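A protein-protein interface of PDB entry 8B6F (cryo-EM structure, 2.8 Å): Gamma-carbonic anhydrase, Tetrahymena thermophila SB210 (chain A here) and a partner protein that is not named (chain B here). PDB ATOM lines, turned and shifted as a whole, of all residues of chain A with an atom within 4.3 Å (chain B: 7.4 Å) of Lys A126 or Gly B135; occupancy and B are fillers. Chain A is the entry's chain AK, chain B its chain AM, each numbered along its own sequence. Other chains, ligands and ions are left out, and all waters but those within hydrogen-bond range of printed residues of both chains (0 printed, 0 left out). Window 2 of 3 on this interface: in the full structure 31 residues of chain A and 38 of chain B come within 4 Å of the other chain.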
ATOM      1  N   GLU A  97      -1.657  -3.780  18.212  1.00  0.00           N
ATOM      2  CA  GLU A  97      -0.580  -4.631  17.730  1.00  0.00           C
ATOM      3  C   GLU A  97      -0.324  -5.776  18.701  1.00  0.00           C
ATOM      4  O   GLU A  97      -0.445  -5.622  19.918  1.00  0.00           O
ATOM      5  CB  GLU A  97       0.702  -3.818  17.539  1.00  0.00           C
ATOM      6  CG  GLU A  97       0.559  -2.702  16.521  1.00  0.00           C
ATOM      7  CD  GLU A  97       1.789  -1.827  16.434  1.00  0.00           C
ATOM      8  OE1 GLU A  97       2.721  -2.028  17.239  1.00  0.00           O
ATOM      9  OE2 GLU A  97       1.827  -0.939  15.558  1.00  0.00           O
ATOM     10  N   ASN A  98       0.036  -6.931  18.144  1.00  0.00           N
ATOM     11  CA  ASN A  98       0.311  -8.132  18.931  1.00  0.00           C
ATOM     12  C   ASN A  98      -0.900  -8.545  19.763  1.00  0.00           C
ATOM     13  O   ASN A  98      -0.758  -9.129  20.839  1.00  0.00           O
ATOM     14  CB  ASN A  98       1.530  -7.930  19.834  1.00  0.00           C
ATOM     15  CG  ASN A  98       2.761  -7.497  19.063  1.00  0.00           C
ATOM     16  OD1 ASN A  98       2.949  -7.875  17.909  1.00  0.00           O
ATOM     17  ND2 ASN A  98       3.604  -6.694  19.697  1.00  0.00           N
ATOM     18  N   VAL A  99      -2.096  -8.256  19.260  1.00  0.00           N
ATOM     19  CA  VAL A  99      -3.350  -8.556  19.942  1.00  0.00           C
ATOM     20  C   VAL A  99      -3.941  -9.820  19.340  1.00  0.00           C
ATOM     21  O   VAL A  99      -3.962  -9.984  18.114  1.00  0.00           O
ATOM     22  CB  VAL A  99      -4.332  -7.373  19.833  1.00  0.00           C
ATOM     23  CG1 VAL A  99      -5.704  -7.749  20.373  1.00  0.00           C
ATOM     24  CG2 VAL A  99      -3.777  -6.163  20.562  1.00  0.00           C
ATOM     25  N   GLY A 124      -5.774  -2.193  23.371  1.00  0.00           N
ATOM     26  CA  GLY A 124      -4.351  -1.946  23.424  1.00  0.00           C
ATOM     27  C   GLY A 124      -3.539  -3.126  22.928  1.00  0.00           C
ATOM     28  O   GLY A 124      -4.016  -4.255  22.821  1.00  0.00           O
ATOM     29  N   SER A 125      -2.276  -2.849  22.624  1.00  0.00           N
ATOM     30  CA  SER A 125      -1.389  -3.881  22.118  1.00  0.00           C
ATOM     31  C   SER A 125      -1.081  -4.908  23.206  1.00  0.00           C
ATOM     32  O   SER A 125      -1.223  -4.648  24.403  1.00  0.00           O
ATOM     33  CB  SER A 125      -0.095  -3.258  21.598  1.00  0.00           C
ATOM     34  OG  SER A 125       0.511  -2.449  22.588  1.00  0.00           O
ATOM     35  N   LYS A 126      -0.661  -6.096  22.771  1.00  0.00           N
ATOM     36  CA  LYS A 126      -0.263  -7.207  23.631  1.00  0.00           C
ATOM     37  C   LYS A 126      -1.443  -7.842  24.357  1.00  0.00           C
ATOM     38  O   LYS A 126      -1.244  -8.728  25.194  1.00  0.00           O
ATOM     39  CB  LYS A 126       0.805  -6.758  24.642  1.00  0.00           C
ATOM     40  CG  LYS A 126       1.336  -7.827  25.600  1.00  0.00           C
ATOM     41  CD  LYS A 126       1.776  -9.094  24.888  1.00  0.00           C
ATOM     42  CE  LYS A 126       2.289 -10.115  25.894  1.00  0.00           C
ATOM     43  NZ  LYS A 126       2.738 -11.379  25.244  1.00  0.00           N
ATOM     44  N   SER A 127      -2.668  -7.448  24.035  1.00  0.00           N
ATOM     45  CA  SER A 127      -3.843  -7.917  24.755  1.00  0.00           C
ATOM     46  C   SER A 127      -4.436  -9.156  24.092  1.00  0.00           C
ATOM     47  O   SER A 127      -4.231  -9.419  22.906  1.00  0.00           O
ATOM     48  CB  SER A 127      -4.893  -6.811  24.848  1.00  0.00           C
ATOM     49  OG  SER A 127      -5.144  -6.237  23.585  1.00  0.00           O
ATOM     50  N   THR A 128      -5.182  -9.922  24.885  1.00  0.00           N
ATOM     51  CA  THR A 128      -5.845 -11.134  24.424  1.00  0.00           C
ATOM     52  C   THR A 128      -7.323 -11.047  24.768  1.00  0.00           C
ATOM     53  O   THR A 128      -7.681 -10.757  25.913  1.00  0.00           O
ATOM     54  CB  THR A 128      -5.231 -12.382  25.059  1.00  0.00           C
ATOM     55  OG1 THR A 128      -3.809 -12.233  25.139  1.00  0.00           O
ATOM     56  CG2 THR A 128      -5.549 -13.609  24.221  1.00  0.00           C
ATOM     57  N   GLY A 143      -1.786  -5.027  26.987  1.00  0.00           N
ATOM     58  CA  GLY A 143      -1.477  -6.216  27.751  1.00  0.00           C
ATOM     59  C   GLY A 143      -2.623  -6.777  28.562  1.00  0.00           C
ATOM     60  O   GLY A 143      -2.385  -7.630  29.425  1.00  0.00           O
ATOM     61  N   SER B  87       8.495  -7.651  15.962  1.00  0.00           N
ATOM     62  CA  SER B  87       8.341  -6.356  16.605  1.00  0.00           C
ATOM     63  C   SER B  87       8.093  -5.285  15.554  1.00  0.00           C
ATOM     64  O   SER B  87       8.689  -5.303  14.476  1.00  0.00           O
ATOM     65  CB  SER B  87       9.583  -6.014  17.427  1.00  0.00           C
ATOM     66  OG  SER B  87      10.743  -6.021  16.617  1.00  0.00           O
ATOM     67  N   GLY B 105      13.456  -6.725  21.833  1.00  0.00           N
ATOM     68  CA  GLY B 105      13.047  -8.112  21.832  1.00  0.00           C
ATOM     69  C   GLY B 105      11.953  -8.396  20.823  1.00  0.00           C
ATOM     70  O   GLY B 105      11.379  -7.506  20.196  1.00  0.00           O
ATOM     71  N   ASP B 106      11.673  -9.684  20.658  1.00  0.00           N
ATOM     72  CA  ASP B 106      10.642 -10.112  19.727  1.00  0.00           C
ATOM     73  C   ASP B 106       9.266  -9.678  20.216  1.00  0.00           C
ATOM     74  O   ASP B 106       8.989  -9.668  21.418  1.00  0.00           O
ATOM     75  CB  ASP B 106      10.681 -11.629  19.558  1.00  0.00           C
ATOM     76  CG  ASP B 106      12.069 -12.140  19.220  1.00  0.00           C
ATOM     77  OD1 ASP B 106      12.953 -12.080  20.099  1.00  0.00           O
ATOM     78  OD2 ASP B 106      12.275 -12.604  18.081  1.00  0.00           O
ATOM     79  N   LYS B 107       8.400  -9.310  19.274  1.00  0.00           N
ATOM     80  CA  LYS B 107       7.017  -8.941  19.548  1.00  0.00           C
ATOM     81  C   LYS B 107       6.895  -7.625  20.306  1.00  0.00           C
ATOM     82  O   LYS B 107       5.833  -7.326  20.859  1.00  0.00           O
ATOM     83  CB  LYS B 107       6.301 -10.057  20.321  1.00  0.00           C
ATOM     84  CG  LYS B 107       4.781  -9.979  20.266  1.00  0.00           C
ATOM     85  CD  LYS B 107       4.134 -11.263  20.764  1.00  0.00           C
ATOM     86  CE  LYS B 107       4.460 -11.524  22.221  1.00  0.00           C
ATOM     87  NZ  LYS B 107       3.747 -12.721  22.740  1.00  0.00           N
ATOM     88  N   VAL B 108       7.953  -6.824  20.353  1.00  0.00           N
ATOM     89  CA  VAL B 108       7.881  -5.508  20.975  1.00  0.00           C
ATOM     90  C   VAL B 108       7.141  -4.554  20.050  1.00  0.00           C
ATOM     91  O   VAL B 108       7.359  -4.548  18.833  1.00  0.00           O
ATOM     92  CB  VAL B 108       9.291  -4.984  21.301  1.00  0.00           C
ATOM     93  CG1 VAL B 108       9.241  -3.524  21.738  1.00  0.00           C
ATOM     94  CG2 VAL B 108       9.936  -5.835  22.375  1.00  0.00           C
ATOM     95  N   ALA B 109       6.252  -3.749  20.624  1.00  0.00           N
ATOM     96  CA  ALA B 109       5.469  -2.779  19.874  1.00  0.00           C
ATOM     97  C   ALA B 109       5.791  -1.382  20.383  1.00  0.00           C
ATOM     98  O   ALA B 109       5.710  -1.127  21.588  1.00  0.00           O
ATOM     99  CB  ALA B 109       3.972  -3.060  20.008  1.00  0.00           C
ATOM    100  N   ILE B 132      15.584  -4.244  25.756  1.00  0.00           N
ATOM    101  CA  ILE B 132      14.140  -4.318  25.945  1.00  0.00           C
ATOM    102  C   ILE B 132      13.702  -5.746  25.655  1.00  0.00           C
ATOM    103  O   ILE B 132      13.972  -6.278  24.571  1.00  0.00           O
ATOM    104  CB  ILE B 132      13.408  -3.315  25.045  1.00  0.00           C
ATOM    105  CG1 ILE B 132      14.039  -1.930  25.219  1.00  0.00           C
ATOM    106  CG2 ILE B 132      11.922  -3.299  25.379  1.00  0.00           C
ATOM    107  CD1 ILE B 132      13.355  -0.822  24.472  1.00  0.00           C
ATOM    108  N   GLY B 133      13.023  -6.361  26.616  1.00  0.00           N
ATOM    109  CA  GLY B 133      12.626  -7.745  26.480  1.00  0.00           C
ATOM    110  C   GLY B 133      11.495  -7.933  25.490  1.00  0.00           C
ATOM    111  O   GLY B 133      10.851  -6.990  25.028  1.00  0.00           O
ATOM    112  N   ALA B 134      11.251  -9.197  25.160  1.00  0.00           N
ATOM    113  CA  ALA B 134      10.192  -9.537  24.222  1.00  0.00           C
ATOM    114  C   ALA B 134       8.823  -9.276  24.839  1.00  0.00           C
ATOM    115  O   ALA B 134       8.614  -9.448  26.041  1.00  0.00           O
ATOM    116  CB  ALA B 134      10.305 -11.002  23.801  1.00  0.00           C
ATOM    117  N   GLY B 135       7.885  -8.854  23.994  1.00  0.00           N
ATOM    118  CA  GLY B 135       6.527  -8.609  24.433  1.00  0.00           C
ATOM    119  C   GLY B 135       6.298  -7.286  25.123  1.00  0.00           C
ATOM    120  O   GLY B 135       5.236  -7.100  25.726  1.00  0.00           O
ATOM    121  N   CYS B 136       7.255  -6.365  25.064  1.00  0.00           N
ATOM    122  CA  CYS B 136       7.098  -5.065  25.695  1.00  0.00           C
ATOM    123  C   CYS B 136       6.291  -4.125  24.806  1.00  0.00           C
ATOM    124  O   CYS B 136       6.210  -4.289  23.586  1.00  0.00           O
ATOM    125  CB  CYS B 136       8.463  -4.442  25.986  1.00  0.00           C
ATOM    126  SG  CYS B 136       9.422  -5.297  27.245  1.00  0.00           S
ATOM    127  N   VAL B 137       5.684  -3.125  25.441  1.00  0.00           N
ATOM    128  CA  VAL B 137       4.946  -2.073  24.752  1.00  0.00           C
ATOM    129  C   VAL B 137       5.486  -0.733  25.228  1.00  0.00           C
ATOM    130  O   VAL B 137       5.661  -0.524  26.434  1.00  0.00           O
ATOM    131  CB  VAL B 137       3.429  -2.173  25.007  1.00  0.00           C
ATOM    132  CG1 VAL B 137       2.689  -1.064  24.277  1.00  0.00           C
ATOM    133  CG2 VAL B 137       2.908  -3.532  24.573  1.00  0.00           C
ATOM    134  N   GLY B 150      12.323  -5.449  31.501  1.00  0.00           N
ATOM    135  CA  GLY B 150      11.966  -6.849  31.484  1.00  0.00           C
ATOM    136  C   GLY B 150      10.890  -7.161  30.462  1.00  0.00           C
ATOM    137  O   GLY B 150      10.199  -6.282  29.948  1.00  0.00           O
ATOM    138  N   HIS B 151      10.753  -8.449  30.165  1.00  0.00           N
ATOM    139  CA  HIS B 151       9.773  -8.894  29.187  1.00  0.00           C
ATOM    140  C   HIS B 151       8.359  -8.599  29.671  1.00  0.00           C
ATOM    141  O   HIS B 151       8.078  -8.581  30.873  1.00  0.00           O
ATOM    142  CB  HIS B 151       9.929 -10.393  28.922  1.00  0.00           C
ATOM    143  CG  HIS B 151       9.755 -11.242  30.143  1.00  0.00           C
ATOM    144  ND1 HIS B 151      10.818 -11.686  30.900  1.00  0.00           N
ATOM    145  CD2 HIS B 151       8.641 -11.726  30.741  1.00  0.00           C
ATOM    146  CE1 HIS B 151      10.367 -12.407  31.910  1.00  0.00           C
ATOM    147  NE2 HIS B 151       9.049 -12.447  31.837  1.00  0.00           N
ATOM    148  N   ASN B 152       7.459  -8.360  28.716  1.00  0.00           N
ATOM    149  CA  ASN B 152       6.051  -8.100  29.009  1.00  0.00           C
ATOM    150  C   ASN B 152       5.893  -6.891  29.929  1.00  0.00           C
ATOM    151  O   ASN B 152       5.169  -6.928  30.925  1.00  0.00           O
ATOM    152  CB  ASN B 152       5.382  -9.334  29.615  1.00  0.00           C
ATOM    153  CG  ASN B 152       5.363 -10.510  28.666  1.00  0.00           C
ATOM    154  OD1 ASN B 152       6.116 -10.553  27.696  1.00  0.00           O
ATOM    155  ND2 ASN B 152       4.497 -11.478  28.941  1.00  0.00           N
ATOM    156  N   THR B 153       6.579  -5.808  29.581  1.00  0.00           N
ATOM    157  CA  THR B 153       6.533  -4.563  30.332  1.00  0.00           C
ATOM    158  C   THR B 153       5.895  -3.478  29.477  1.00  0.00           C
ATOM    159  O   THR B 153       6.165  -3.381  28.277  1.00  0.00           O
ATOM    160  CB  THR B 153       7.935  -4.128  30.775  1.00  0.00           C
ATOM    161  OG1 THR B 153       8.385  -4.966  31.845  1.00  0.00           O
ATOM    162  CG2 THR B 153       7.946  -2.673  31.247  1.00  0.00           C
ATOM    163  N   VAL B 154       5.045  -2.668  30.100  1.00  0.00           N
ATOM    164  CA  VAL B 154       4.318  -1.602  29.424  1.00  0.00           C
ATOM    165  C   VAL B 154       4.841  -0.272  29.945  1.00  0.00           C
ATOM    166  O   VAL B 154       4.880  -0.045  31.159  1.00  0.00           O
ATOM    167  CB  VAL B 154       2.801  -1.725  29.643  1.00  0.00           C
ATOM    168  CG1 VAL B 154       2.059  -0.625  28.898  1.00  0.00           C
ATOM    169  CG2 VAL B 154       2.311  -3.090  29.194  1.00  0.00           C
ATOM    170  N   ASN B 170       6.905  -8.079  33.467  1.00  0.00           N
ATOM    171  CA  ASN B 170       5.494  -8.144  33.848  1.00  0.00           C
ATOM    172  C   ASN B 170       5.109  -6.974  34.749  1.00  0.00           C
ATOM    173  O   ASN B 170       4.318  -7.121  35.682  1.00  0.00           O
ATOM    174  CB  ASN B 170       5.167  -9.478  34.521  1.00  0.00           C
ATOM    175  CG  ASN B 170       5.607 -10.663  33.695  1.00  0.00           C
ATOM    176  OD1 ASN B 170       6.463 -11.443  34.110  1.00  0.00           O
ATOM    177  ND2 ASN B 170       5.025 -10.805  32.513  1.00  0.00           N
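The side-chain amide nitrogen of Asn A98 lies within hydrogen-bond range of the backbone carbonyl oxygen of Lys B107, at 2.6 Å. NZ of Lys A126 lies close to NZ of Lys B107, at 3.0 Å.
N of Gly A143 lies within hydrogen-bond range of O of Ser A125, 2.7 Å away. The backbone NH (N) of Gly B135 is in hydrogen-bond range of the backbone carbonyl oxygen (O) of Asp B106. The backbone NH (N) of Lys A126 sits at hydrogen-bond distance from the backbone carbonyl oxygen (O) of Glu A97 (2.9 Å). The backbone NH of Ala B109 lies within hydrogen-bond range of the backbone carbonyl oxygen of Cys B136, at 3.0 Å. The backbone NH (N) of Val B137 is in hydrogen-bond range of the backbone carbonyl oxygen (O) of Thr B153 (2.9 Å).
Ala B109 touches Glu A97. Asn A98 touches Ala B109 (ND2 to CB, 3.7 Å). Val B137 touches Ser A125 (CG1 to OG, 3.1 Å). Lys A126 touches Gly B135. Lys A126 touches Val B137 (CB to CG2, 3.9 Å).
Of the printed residues of chain B, Lys A126 touches Lys B107, Gly B135 and Val B137. Of the printed residues of chain A, Gly B135 touches Lys A126 (3.97 Å). Of the printed residues of chain A, Val B137 touches Ser A125 and Lys A126. Of the printed residues of chain A, Lys B107 touches Asn A98 (2.6 Å) and Lys A126 (3.0 Å). Printed residues of chain A within 4 Å of Ala B109: Glu A97 (3.2 Å) and Asn A98 (3.7 Å). Of the printed residues of chain B, Asn A98 touches Lys B107 (2.6 Å) and Ala B109 (3.7 Å). Ile B132 touches none of the printed residues of chain A. The nearest printed residue of chain A that does not touch Gly B135 is Asn A98 (5.9 Å). The nearest printed residue of chain B that does not touch Glu A97 is Val B108 (5.5 Å).
Printed residues of chain B that touch a printed residue of chain A: Lys B107, Ala B109, Gly B135 and Val B137. Hydrophobic or aromatic side chains of chain B that line the printed part of chain A: Ala B109 and Val B137. Printed residues of chain A that touch a printed residue of chain B: Glu A97, Asn A98, Ser A125 and Lys A126. Among the printed residues, 7 pairs touch across the chains. Among the printed residues, no Asp or Glu carboxylate lies within 4 Å of a Lys or Arg side-chain nitrogen of the other chain.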
